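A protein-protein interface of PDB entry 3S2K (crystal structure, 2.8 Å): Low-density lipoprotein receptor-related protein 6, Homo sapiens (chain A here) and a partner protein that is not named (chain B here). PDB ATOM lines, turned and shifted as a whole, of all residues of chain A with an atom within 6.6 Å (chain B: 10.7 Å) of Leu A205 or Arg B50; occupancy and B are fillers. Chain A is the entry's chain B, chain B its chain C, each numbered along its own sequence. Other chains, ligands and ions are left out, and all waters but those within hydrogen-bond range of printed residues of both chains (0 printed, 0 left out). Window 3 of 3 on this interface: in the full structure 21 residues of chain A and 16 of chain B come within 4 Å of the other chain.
Thr A185 touches three residues of chain B.
Asn A186 touches one residue of chain B.
No residue of chain B comes within 4 Å of Ile A188.
No residue of chain B comes within 4 Å of Ala A202.
Of chain B, only Arg B50 comes within 4 Å of Leu A205.
No residue of chain B comes within 4 Å of Pro A206.
Asp A222 touches none of the printed residues of chain B.
Arg B50 touches three residues of chain A.
Gly B56 touches none of the printed residues of chain A.
Printed residues of chain A within 4 Å of Arg B85: Thr A185 (3.4 Å).
Printed residues of chain A within 4 Å of Leu B86: Thr A185.
Thr A185 touches Arg B85.
CD1 of Leu B86 touches CG2 of Thr A185 (3.5 Å).
Leu A205 touches Arg B50.
The side-chain amide nitrogen (ND2) of Asn A186 sits at hydrogen-bond distance from the backbone carbonyl oxygen (O) of Pro A206 (3.2 Å).
Printed residues of chain A that touch a printed residue of chain B: Thr A185, Asn A186 and Leu A205.
Of the 17 printed residues of chain B, 3 touch a printed residue of chain A.
Hydrophobic or aromatic side chains of chain B that line the printed part of chain A: Leu B86.
Among the printed residues, no Asp or Glu carboxylate lies within 4 Å of a Lys or Arg side-chain nitrogen of the other chain.
The guanidinium group (NE) of Arg B50 is in hydrogen-bond range of the side-chain amide oxygen (OD1) of Asn A186 (3.4 Å).
The guanidinium group (NH2) of Arg B50 sits at hydrogen-bond distance from the backbone carbonyl oxygen (O) of Thr A185 (3.0 Å).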
ATOM      1  N   ASP A 184      10.940  27.074   9.451  1.00  0.00           N
ATOM      2  CA  ASP A 184      11.103  28.470   9.044  1.00  0.00           C
ATOM      3  C   ASP A 184       9.794  29.096   8.568  1.00  0.00           C
ATOM      4  O   ASP A 184       9.638  30.315   8.598  1.00  0.00           O
ATOM      5  CB  ASP A 184      12.185  28.604   7.965  1.00  0.00           C
ATOM      6  CG  ASP A 184      13.581  28.314   8.499  1.00  0.00           C
ATOM      7  OD1 ASP A 184      14.284  27.455   7.922  1.00  0.00           O
ATOM      8  OD2 ASP A 184      13.981  28.950   9.496  1.00  0.00           O
ATOM      9  N   THR A 185       8.858  28.259   8.131  1.00  0.00           N
ATOM     10  CA  THR A 185       7.561  28.742   7.664  1.00  0.00           C
ATOM     11  C   THR A 185       6.407  28.135   8.459  1.00  0.00           C
ATOM     12  O   THR A 185       5.239  28.320   8.118  1.00  0.00           O
ATOM     13  CB  THR A 185       7.355  28.461   6.165  1.00  0.00           C
ATOM     14  OG1 THR A 185       7.567  27.070   5.900  1.00  0.00           O
ATOM     15  CG2 THR A 185       8.331  29.281   5.338  1.00  0.00           C
ATOM     16  N   ASN A 186       6.749  27.405   9.516  1.00  0.00           N
ATOM     17  CA  ASN A 186       5.762  26.878  10.456  1.00  0.00           C
ATOM     18  C   ASN A 186       4.587  26.153   9.809  1.00  0.00           C
ATOM     19  O   ASN A 186       3.435  26.367  10.185  1.00  0.00           O
ATOM     20  CB  ASN A 186       5.238  27.999  11.357  1.00  0.00           C
ATOM     21  CG  ASN A 186       6.336  28.668  12.150  1.00  0.00           C
ATOM     22  OD1 ASN A 186       6.557  29.874  12.032  1.00  0.00           O
ATOM     23  ND2 ASN A 186       7.038  27.887  12.963  1.00  0.00           N
ATOM     24  N   LEU A 187       4.873  25.290   8.843  1.00  0.00           N
ATOM     25  CA  LEU A 187       3.810  24.524   8.207  1.00  0.00           C
ATOM     26  C   LEU A 187       4.189  23.067   7.953  1.00  0.00           C
ATOM     27  O   LEU A 187       5.359  22.696   8.024  1.00  0.00           O
ATOM     28  CB  LEU A 187       3.337  25.208   6.917  1.00  0.00           C
ATOM     29  CG  LEU A 187       4.386  25.883   6.038  1.00  0.00           C
ATOM     30  CD1 LEU A 187       5.422  24.880   5.567  1.00  0.00           C
ATOM     31  CD2 LEU A 187       3.714  26.554   4.858  1.00  0.00           C
ATOM     32  N   ILE A 188       3.175  22.249   7.683  1.00  0.00           N
ATOM     33  CA  ILE A 188       3.366  20.841   7.369  1.00  0.00           C
ATOM     34  C   ILE A 188       3.023  20.595   5.910  1.00  0.00           C
ATOM     35  O   ILE A 188       1.881  20.786   5.492  1.00  0.00           O
ATOM     36  CB  ILE A 188       2.473  19.944   8.236  1.00  0.00           C
ATOM     37  CG1 ILE A 188       2.831  20.098   9.715  1.00  0.00           C
ATOM     38  CG2 ILE A 188       2.600  18.490   7.799  1.00  0.00           C
ATOM     39  CD1 ILE A 188       2.023  19.199  10.630  1.00  0.00           C
ATOM     40  N   ALA A 202      -1.074  21.879   6.502  1.00  0.00           N
ATOM     41  CA  ALA A 202      -1.471  22.780   7.582  1.00  0.00           C
ATOM     42  C   ALA A 202      -0.539  23.985   7.665  1.00  0.00           C
ATOM     43  O   ALA A 202       0.679  23.834   7.621  1.00  0.00           O
ATOM     44  CB  ALA A 202      -1.491  22.036   8.905  1.00  0.00           C
ATOM     45  N   ASP A 203      -1.110  25.179   7.795  1.00  0.00           N
ATOM     46  CA  ASP A 203      -0.306  26.400   7.804  1.00  0.00           C
ATOM     47  C   ASP A 203      -0.476  27.241   9.067  1.00  0.00           C
ATOM     48  O   ASP A 203       0.434  27.974   9.458  1.00  0.00           O
ATOM     49  CB  ASP A 203      -0.612  27.250   6.569  1.00  0.00           C
ATOM     50  CG  ASP A 203      -2.030  27.782   6.567  1.00  0.00           C
ATOM     51  OD1 ASP A 203      -2.296  28.769   5.850  1.00  0.00           O
ATOM     52  OD2 ASP A 203      -2.882  27.217   7.285  1.00  0.00           O
ATOM     53  N   ASP A 204      -1.641  27.140   9.698  1.00  0.00           N
ATOM     54  CA  ASP A 204      -1.926  27.936  10.889  1.00  0.00           C
ATOM     55  C   ASP A 204      -1.332  27.321  12.158  1.00  0.00           C
ATOM     56  O   ASP A 204      -1.984  27.273  13.200  1.00  0.00           O
ATOM     57  CB  ASP A 204      -3.434  28.158  11.045  1.00  0.00           C
ATOM     58  CG  ASP A 204      -4.234  26.873  10.923  1.00  0.00           C
ATOM     59  OD1 ASP A 204      -5.383  26.841  11.416  1.00  0.00           O
ATOM     60  OD2 ASP A 204      -3.718  25.896  10.335  1.00  0.00           O
ATOM     61  N   LEU A 205      -0.088  26.859  12.064  1.00  0.00           N
ATOM     62  CA  LEU A 205       0.582  26.236  13.200  1.00  0.00           C
ATOM     63  C   LEU A 205       1.695  27.133  13.731  1.00  0.00           C
ATOM     64  O   LEU A 205       2.531  27.610  12.966  1.00  0.00           O
ATOM     65  CB  LEU A 205       1.146  24.870  12.808  1.00  0.00           C
ATOM     66  CG  LEU A 205       0.188  23.898  12.114  1.00  0.00           C
ATOM     67  CD1 LEU A 205       0.892  22.586  11.797  1.00  0.00           C
ATOM     68  CD2 LEU A 205      -1.049  23.652  12.960  1.00  0.00           C
ATOM     69  N   PRO A 206       1.706  27.364  15.052  1.00  0.00           N
ATOM     70  CA  PRO A 206       2.661  28.281  15.683  1.00  0.00           C
ATOM     71  C   PRO A 206       4.104  27.783  15.684  1.00  0.00           C
ATOM     72  O   PRO A 206       5.006  28.565  15.379  1.00  0.00           O
ATOM     73  CB  PRO A 206       2.138  28.402  17.120  1.00  0.00           C
ATOM     74  CG  PRO A 206       1.339  27.177  17.343  1.00  0.00           C
ATOM     75  CD  PRO A 206       0.738  26.819  16.018  1.00  0.00           C
ATOM     76  N   HIS A 207       4.327  26.515  16.017  1.00  0.00           N
ATOM     77  CA  HIS A 207       5.692  26.016  16.162  1.00  0.00           C
ATOM     78  C   HIS A 207       5.789  24.503  15.984  1.00  0.00           C
ATOM     79  O   HIS A 207       6.171  23.788  16.912  1.00  0.00           O
ATOM     80  CB  HIS A 207       6.242  26.416  17.534  1.00  0.00           C
ATOM     81  CG  HIS A 207       7.734  26.540  17.576  1.00  0.00           C
ATOM     82  ND1 HIS A 207       8.575  25.486  17.304  1.00  0.00           N
ATOM     83  CD2 HIS A 207       8.528  27.598  17.866  1.00  0.00           C
ATOM     84  CE1 HIS A 207       9.831  25.889  17.422  1.00  0.00           C
ATOM     85  NE2 HIS A 207       9.828  27.163  17.760  1.00  0.00           N
ATOM     86  N   PRO A 208       5.458  24.009  14.782  1.00  0.00           N
ATOM     87  CA  PRO A 208       5.495  22.566  14.523  1.00  0.00           C
ATOM     88  C   PRO A 208       6.931  22.064  14.524  1.00  0.00           C
ATOM     89  O   PRO A 208       7.818  22.774  14.056  1.00  0.00           O
ATOM     90  CB  PRO A 208       4.903  22.443  13.111  1.00  0.00           C
ATOM     91  CG  PRO A 208       4.286  23.773  12.812  1.00  0.00           C
ATOM     92  CD  PRO A 208       5.080  24.770  13.584  1.00  0.00           C
ATOM     93  N   TRP A 220       1.879  15.431  14.805  1.00  0.00           N
ATOM     94  CA  TRP A 220       3.027  16.320  14.938  1.00  0.00           C
ATOM     95  C   TRP A 220       3.149  16.878  16.349  1.00  0.00           C
ATOM     96  O   TRP A 220       2.230  16.764  17.160  1.00  0.00           O
ATOM     97  CB  TRP A 220       2.959  17.463  13.919  1.00  0.00           C
ATOM     98  CG  TRP A 220       1.904  18.494  14.213  1.00  0.00           C
ATOM     99  CD1 TRP A 220       2.064  19.657  14.911  1.00  0.00           C
ATOM    100  CD2 TRP A 220       0.530  18.458  13.809  1.00  0.00           C
ATOM    101  NE1 TRP A 220       0.876  20.343  14.969  1.00  0.00           N
ATOM    102  CE2 TRP A 220      -0.083  19.626  14.299  1.00  0.00           C
ATOM    103  CE3 TRP A 220      -0.242  17.546  13.081  1.00  0.00           C
ATOM    104  CZ2 TRP A 220      -1.429  19.911  14.088  1.00  0.00           C
ATOM    105  CZ3 TRP A 220      -1.578  17.829  12.871  1.00  0.00           C
ATOM    106  CH2 TRP A 220      -2.158  19.001  13.372  1.00  0.00           C
ATOM    107  N   ASP A 222       4.335  20.384  18.798  1.00  0.00           N
ATOM    108  CA  ASP A 222       4.418  21.831  18.728  1.00  0.00           C
ATOM    109  C   ASP A 222       5.051  22.371  19.998  1.00  0.00           C
ATOM    110  O   ASP A 222       4.514  22.203  21.093  1.00  0.00           O
ATOM    111  CB  ASP A 222       3.038  22.448  18.499  1.00  0.00           C
ATOM    112  CG  ASP A 222       3.100  23.946  18.260  1.00  0.00           C
ATOM    113  OD1 ASP A 222       3.649  24.673  19.117  1.00  0.00           O
ATOM    114  OD2 ASP A 222       2.605  24.396  17.206  1.00  0.00           O
ATOM    115  N   ARG A 225       2.770  25.250  21.722  1.00  0.00           N
ATOM    116  CA  ARG A 225       1.549  24.788  22.367  1.00  0.00           C
ATOM    117  C   ARG A 225       1.809  23.562  23.235  1.00  0.00           C
ATOM    118  O   ARG A 225       0.878  22.984  23.798  1.00  0.00           O
ATOM    119  CB  ARG A 225       0.458  24.512  21.327  1.00  0.00           C
ATOM    120  CG  ARG A 225      -0.021  25.770  20.608  1.00  0.00           C
ATOM    121  CD  ARG A 225      -1.025  25.451  19.516  1.00  0.00           C
ATOM    122  NE  ARG A 225      -2.278  24.927  20.047  1.00  0.00           N
ATOM    123  CZ  ARG A 225      -3.241  24.399  19.298  1.00  0.00           C
ATOM    124  NH1 ARG A 225      -3.091  24.322  17.981  1.00  0.00           N
ATOM    125  NH2 ARG A 225      -4.351  23.944  19.863  1.00  0.00           N
ATOM    126  N   GLU A 229      -0.442  16.818  18.447  1.00  0.00           N
ATOM    127  CA  GLU A 229      -1.733  16.918  17.775  1.00  0.00           C
ATOM    128  C   GLU A 229      -1.772  16.047  16.523  1.00  0.00           C
ATOM    129  O   GLU A 229      -0.726  15.679  15.986  1.00  0.00           O
ATOM    130  CB  GLU A 229      -2.019  18.375  17.407  1.00  0.00           C
ATOM    131  CG  GLU A 229      -1.715  19.362  18.522  1.00  0.00           C
ATOM    132  CD  GLU A 229      -1.936  20.802  18.104  1.00  0.00           C
ATOM    133  OE1 GLU A 229      -1.213  21.687  18.608  1.00  0.00           O
ATOM    134  OE2 GLU A 229      -2.835  21.051  17.276  1.00  0.00           O
ATOM    135  N   ARG A 239      -9.001  18.166  13.224  1.00  0.00           N
ATOM    136  CA  ARG A 239      -7.859  18.227  14.130  1.00  0.00           C
ATOM    137  C   ARG A 239      -8.255  18.045  15.593  1.00  0.00           C
ATOM    138  O   ARG A 239      -9.228  18.632  16.065  1.00  0.00           O
ATOM    139  CB  ARG A 239      -7.105  19.549  13.955  1.00  0.00           C
ATOM    140  CG  ARG A 239      -6.646  19.813  12.529  1.00  0.00           C
ATOM    141  CD  ARG A 239      -5.254  20.427  12.492  1.00  0.00           C
ATOM    142  NE  ARG A 239      -5.261  21.870  12.727  1.00  0.00           N
ATOM    143  CZ  ARG A 239      -5.177  22.783  11.763  1.00  0.00           C
ATOM    144  NH1 ARG A 239      -5.079  22.409  10.493  1.00  0.00           N
ATOM    145  NH2 ARG A 239      -5.190  24.073  12.070  1.00  0.00           N
ATOM    146  N   CYS B  46      17.969  33.005   6.106  1.00  0.00           N
ATOM    147  CA  CYS B  46      18.116  33.525   7.464  1.00  0.00           C
ATOM    148  C   CYS B  46      16.822  33.409   8.272  1.00  0.00           C
ATOM    149  O   CYS B  46      15.745  33.201   7.708  1.00  0.00           O
ATOM    150  CB  CYS B  46      18.625  34.973   7.449  1.00  0.00           C
ATOM    151  SG  CYS B  46      17.625  36.143   6.495  1.00  0.00           S
ATOM    152  N   THR B  47      16.935  33.543   9.591  1.00  0.00           N
ATOM    153  CA  THR B  47      15.797  33.356  10.491  1.00  0.00           C
ATOM    154  C   THR B  47      14.920  34.600  10.600  1.00  0.00           C
ATOM    155  O   THR B  47      15.421  35.719  10.679  1.00  0.00           O
ATOM    156  CB  THR B  47      16.250  32.935  11.915  1.00  0.00           C
ATOM    157  OG1 THR B  47      17.006  31.719  11.846  1.00  0.00           O
ATOM    158  CG2 THR B  47      15.041  32.725  12.824  1.00  0.00           C
ATOM    159  N   LYS B  48      13.607  34.383  10.600  1.00  0.00           N
ATOM    160  CA  LYS B  48      12.629  35.449  10.803  1.00  0.00           C
ATOM    161  C   LYS B  48      11.545  34.972  11.765  1.00  0.00           C
ATOM    162  O   LYS B  48      10.723  34.123  11.408  1.00  0.00           O
ATOM    163  CB  LYS B  48      11.997  35.857   9.473  1.00  0.00           C
ATOM    164  CG  LYS B  48      10.754  36.718   9.614  1.00  0.00           C
ATOM    165  CD  LYS B  48      11.104  38.138  10.010  1.00  0.00           C
ATOM    166  CE  LYS B  48       9.863  39.008  10.098  1.00  0.00           C
ATOM    167  NZ  LYS B  48      10.212  40.440  10.308  1.00  0.00           N
ATOM    168  N   HIS B  49      11.547  35.513  12.981  1.00  0.00           N
ATOM    169  CA  HIS B  49      10.609  35.076  14.014  1.00  0.00           C
ATOM    170  C   HIS B  49       9.240  35.749  13.888  1.00  0.00           C
ATOM    171  O   HIS B  49       9.150  36.956  13.665  1.00  0.00           O
ATOM    172  CB  HIS B  49      11.192  35.318  15.412  1.00  0.00           C
ATOM    173  CG  HIS B  49      12.432  34.529  15.700  1.00  0.00           C
ATOM    174  ND1 HIS B  49      13.692  35.086  15.680  1.00  0.00           N
ATOM    175  CD2 HIS B  49      12.604  33.221  16.011  1.00  0.00           C
ATOM    176  CE1 HIS B  49      14.587  34.157  15.967  1.00  0.00           C
ATOM    177  NE2 HIS B  49      13.951  33.017  16.171  1.00  0.00           N
ATOM    178  N   ARG B  50       8.178  34.961  14.023  1.00  0.00           N
ATOM    179  CA  ARG B  50       6.823  35.501  14.007  1.00  0.00           C
ATOM    180  C   ARG B  50       6.484  36.091  15.368  1.00  0.00           C
ATOM    181  O   ARG B  50       6.282  37.298  15.505  1.00  0.00           O
ATOM    182  CB  ARG B  50       5.801  34.421  13.651  1.00  0.00           C
ATOM    183  CG  ARG B  50       5.838  33.961  12.207  1.00  0.00           C
ATOM    184  CD  ARG B  50       4.776  32.904  11.962  1.00  0.00           C
ATOM    185  NE  ARG B  50       4.809  32.395  10.595  1.00  0.00           N
ATOM    186  CZ  ARG B  50       3.998  31.448  10.133  1.00  0.00           C
ATOM    187  NH1 ARG B  50       3.089  30.904  10.932  1.00  0.00           N
ATOM    188  NH2 ARG B  50       4.098  31.043   8.874  1.00  0.00           N
ATOM    189  N   ARG B  51       6.422  35.227  16.373  1.00  0.00           N
ATOM    190  CA  ARG B  51       6.142  35.664  17.733  1.00  0.00           C
ATOM    191  C   ARG B  51       7.434  35.927  18.502  1.00  0.00           C
ATOM    192  O   ARG B  51       8.428  35.222  18.329  1.00  0.00           O
ATOM    193  CB  ARG B  51       5.280  34.626  18.459  1.00  0.00           C
ATOM    194  CG  ARG B  51       3.963  34.339  17.752  1.00  0.00           C
ATOM    195  CD  ARG B  51       3.052  33.419  18.551  1.00  0.00           C
ATOM    196  NE  ARG B  51       1.731  33.327  17.934  1.00  0.00           N
ATOM    197  CZ  ARG B  51       0.709  32.649  18.445  1.00  0.00           C
ATOM    198  NH1 ARG B  51       0.852  31.995  19.589  1.00  0.00           N
ATOM    199  NH2 ARG B  51      -0.456  32.625  17.811  1.00  0.00           N
ATOM    200  N   LYS B  52       7.411  36.956  19.342  1.00  0.00           N
ATOM    201  CA  LYS B  52       8.542  37.294  20.194  1.00  0.00           C
ATOM    202  C   LYS B  52       9.011  36.072  20.978  1.00  0.00           C
ATOM    203  O   LYS B  52      10.211  35.828  21.119  1.00  0.00           O
ATOM    204  CB  LYS B  52       8.145  38.421  21.151  1.00  0.00           C
ATOM    205  CG  LYS B  52       9.234  38.866  22.111  1.00  0.00           C
ATOM    206  CD  LYS B  52       9.254  40.386  22.255  1.00  0.00           C
ATOM    207  CE  LYS B  52       7.898  40.945  22.666  1.00  0.00           C
ATOM    208  NZ  LYS B  52       7.531  40.583  24.062  1.00  0.00           N
ATOM    209  N   GLY B  53       8.054  35.294  21.469  1.00  0.00           N
ATOM    210  CA  GLY B  53       8.361  34.111  22.250  1.00  0.00           C
ATOM    211  C   GLY B  53       9.093  33.025  21.484  1.00  0.00           C
ATOM    212  O   GLY B  53       9.835  32.240  22.068  1.00  0.00           O
ATOM    213  N   SER B  54       8.891  32.967  20.174  1.00  0.00           N
ATOM    214  CA  SER B  54       9.522  31.924  19.377  1.00  0.00           C
ATOM    215  C   SER B  54      11.035  32.089  19.405  1.00  0.00           C
ATOM    216  O   SER B  54      11.781  31.145  19.137  1.00  0.00           O
ATOM    217  CB  SER B  54       9.005  31.941  17.938  1.00  0.00           C
ATOM    218  OG  SER B  54       9.564  33.022  17.216  1.00  0.00           O
ATOM    219  N   HIS B  55      11.484  33.295  19.733  1.00  0.00           N
ATOM    220  CA  HIS B  55      12.910  33.561  19.857  1.00  0.00           C
ATOM    221  C   HIS B  55      13.483  32.881  21.098  1.00  0.00           C
ATOM    222  O   HIS B  55      14.600  32.364  21.073  1.00  0.00           O
ATOM    223  CB  HIS B  55      13.174  35.066  19.919  1.00  0.00           C
ATOM    224  CG  HIS B  55      14.628  35.421  19.919  1.00  0.00           C
ATOM    225  ND1 HIS B  55      15.422  35.316  21.040  1.00  0.00           N
ATOM    226  CD2 HIS B  55      15.433  35.882  18.931  1.00  0.00           C
ATOM    227  CE1 HIS B  55      16.652  35.693  20.744  1.00  0.00           C
ATOM    228  NE2 HIS B  55      16.684  36.043  19.470  1.00  0.00           N
ATOM    229  N   GLY B  56      12.714  32.889  22.182  1.00  0.00           N
ATOM    230  CA  GLY B  56      13.144  32.267  23.420  1.00  0.00           C
ATOM    231  C   GLY B  56      13.161  30.752  23.334  1.00  0.00           C
ATOM    232  O   GLY B  56      13.881  30.085  24.077  1.00  0.00           O
ATOM    233  N   LEU B  57      12.368  30.210  22.414  1.00  0.00           N
ATOM    234  CA  LEU B  57      12.207  28.766  22.285  1.00  0.00           C
ATOM    235  C   LEU B  57      13.203  28.157  21.305  1.00  0.00           C
ATOM    236  O   LEU B  57      13.513  26.969  21.384  1.00  0.00           O
ATOM    237  CB  LEU B  57      10.780  28.433  21.843  1.00  0.00           C
ATOM    238  CG  LEU B  57       9.647  28.834  22.790  1.00  0.00           C
ATOM    239  CD1 LEU B  57       8.304  28.749  22.081  1.00  0.00           C
ATOM    240  CD2 LEU B  57       9.654  27.977  24.052  1.00  0.00           C
ATOM    241  N   GLU B  58      13.697  28.974  20.381  1.00  0.00           N
ATOM    242  CA  GLU B  58      14.645  28.508  19.376  1.00  0.00           C
ATOM    243  C   GLU B  58      15.833  27.803  20.019  1.00  0.00           C
ATOM    244  O   GLU B  58      16.511  28.375  20.875  1.00  0.00           O
ATOM    245  CB  GLU B  58      15.140  29.681  18.524  1.00  0.00           C
ATOM    246  CG  GLU B  58      16.013  29.284  17.342  1.00  0.00           C
ATOM    247  CD  GLU B  58      15.264  28.450  16.313  1.00  0.00           C
ATOM    248  OE1 GLU B  58      14.928  27.284  16.615  1.00  0.00           O
ATOM    249  OE2 GLU B  58      15.010  28.966  15.203  1.00  0.00           O
ATOM    250  N   ILE B  73      12.806  39.298   2.817  1.00  0.00           N
ATOM    251  CA  ILE B  73      12.051  38.213   2.207  1.00  0.00           C
ATOM    252  C   ILE B  73      12.395  38.066   0.724  1.00  0.00           C
ATOM    253  O   ILE B  73      12.750  39.041   0.058  1.00  0.00           O
ATOM    254  CB  ILE B  73      10.528  38.414   2.390  1.00  0.00           C
ATOM    255  CG1 ILE B  73       9.778  37.099   2.182  1.00  0.00           C
ATOM    256  CG2 ILE B  73      10.003  39.500   1.459  1.00  0.00           C
ATOM    257  CD1 ILE B  73       8.303  37.188   2.505  1.00  0.00           C
ATOM    258  N   ARG B  85       7.273  30.974   1.949  1.00  0.00           N
ATOM    259  CA  ARG B  85       8.047  32.203   1.803  1.00  0.00           C
ATOM    260  C   ARG B  85       9.217  32.263   2.784  1.00  0.00           C
ATOM    261  O   ARG B  85       9.024  32.373   3.997  1.00  0.00           O
ATOM    262  CB  ARG B  85       7.155  33.435   1.980  1.00  0.00           C
ATOM    263  CG  ARG B  85       6.036  33.554   0.957  1.00  0.00           C
ATOM    264  CD  ARG B  85       5.407  34.939   0.989  1.00  0.00           C
ATOM    265  NE  ARG B  85       4.890  35.282   2.312  1.00  0.00           N
ATOM    266  CZ  ARG B  85       3.623  35.133   2.682  1.00  0.00           C
ATOM    267  NH1 ARG B  85       2.732  34.647   1.828  1.00  0.00           N
ATOM    268  NH2 ARG B  85       3.244  35.472   3.907  1.00  0.00           N
ATOM    269  N   LEU B  86      10.432  32.197   2.245  1.00  0.00           N
ATOM    270  CA  LEU B  86      11.644  32.238   3.056  1.00  0.00           C
ATOM    271  C   LEU B  86      12.264  33.627   3.083  1.00  0.00           C
ATOM    272  O   LEU B  86      11.890  34.509   2.309  1.00  0.00           O
ATOM    273  CB  LEU B  86      12.678  31.245   2.516  1.00  0.00           C
ATOM    274  CG  LEU B  86      12.692  29.815   3.051  1.00  0.00           C
ATOM    275  CD1 LEU B  86      11.294  29.334   3.395  1.00  0.00           C
ATOM    276  CD2 LEU B  86      13.349  28.897   2.035  1.00  0.00           C
ATOM    277  N   HIS B  87      13.223  33.812   3.982  1.00  0.00           N
ATOM    278  CA  HIS B  87      14.008  35.036   4.034  1.00  0.00           C
ATOM    279  C   HIS B  87      15.471  34.718   3.739  1.00  0.00           C
ATOM    280  O   HIS B  87      16.014  33.723   4.228  1.00  0.00           O
ATOM    281  CB  HIS B  87      13.872  35.704   5.403  1.00  0.00           C
ATOM    282  CG  HIS B  87      12.497  36.224   5.684  1.00  0.00           C
ATOM    283  ND1 HIS B  87      12.240  37.559   5.912  1.00  0.00           N
ATOM    284  CD2 HIS B  87      11.303  35.590   5.766  1.00  0.00           C
ATOM    285  CE1 HIS B  87      10.946  37.724   6.125  1.00  0.00           C
ATOM    286  NE2 HIS B  87      10.356  36.545   6.043  1.00  0.00           N
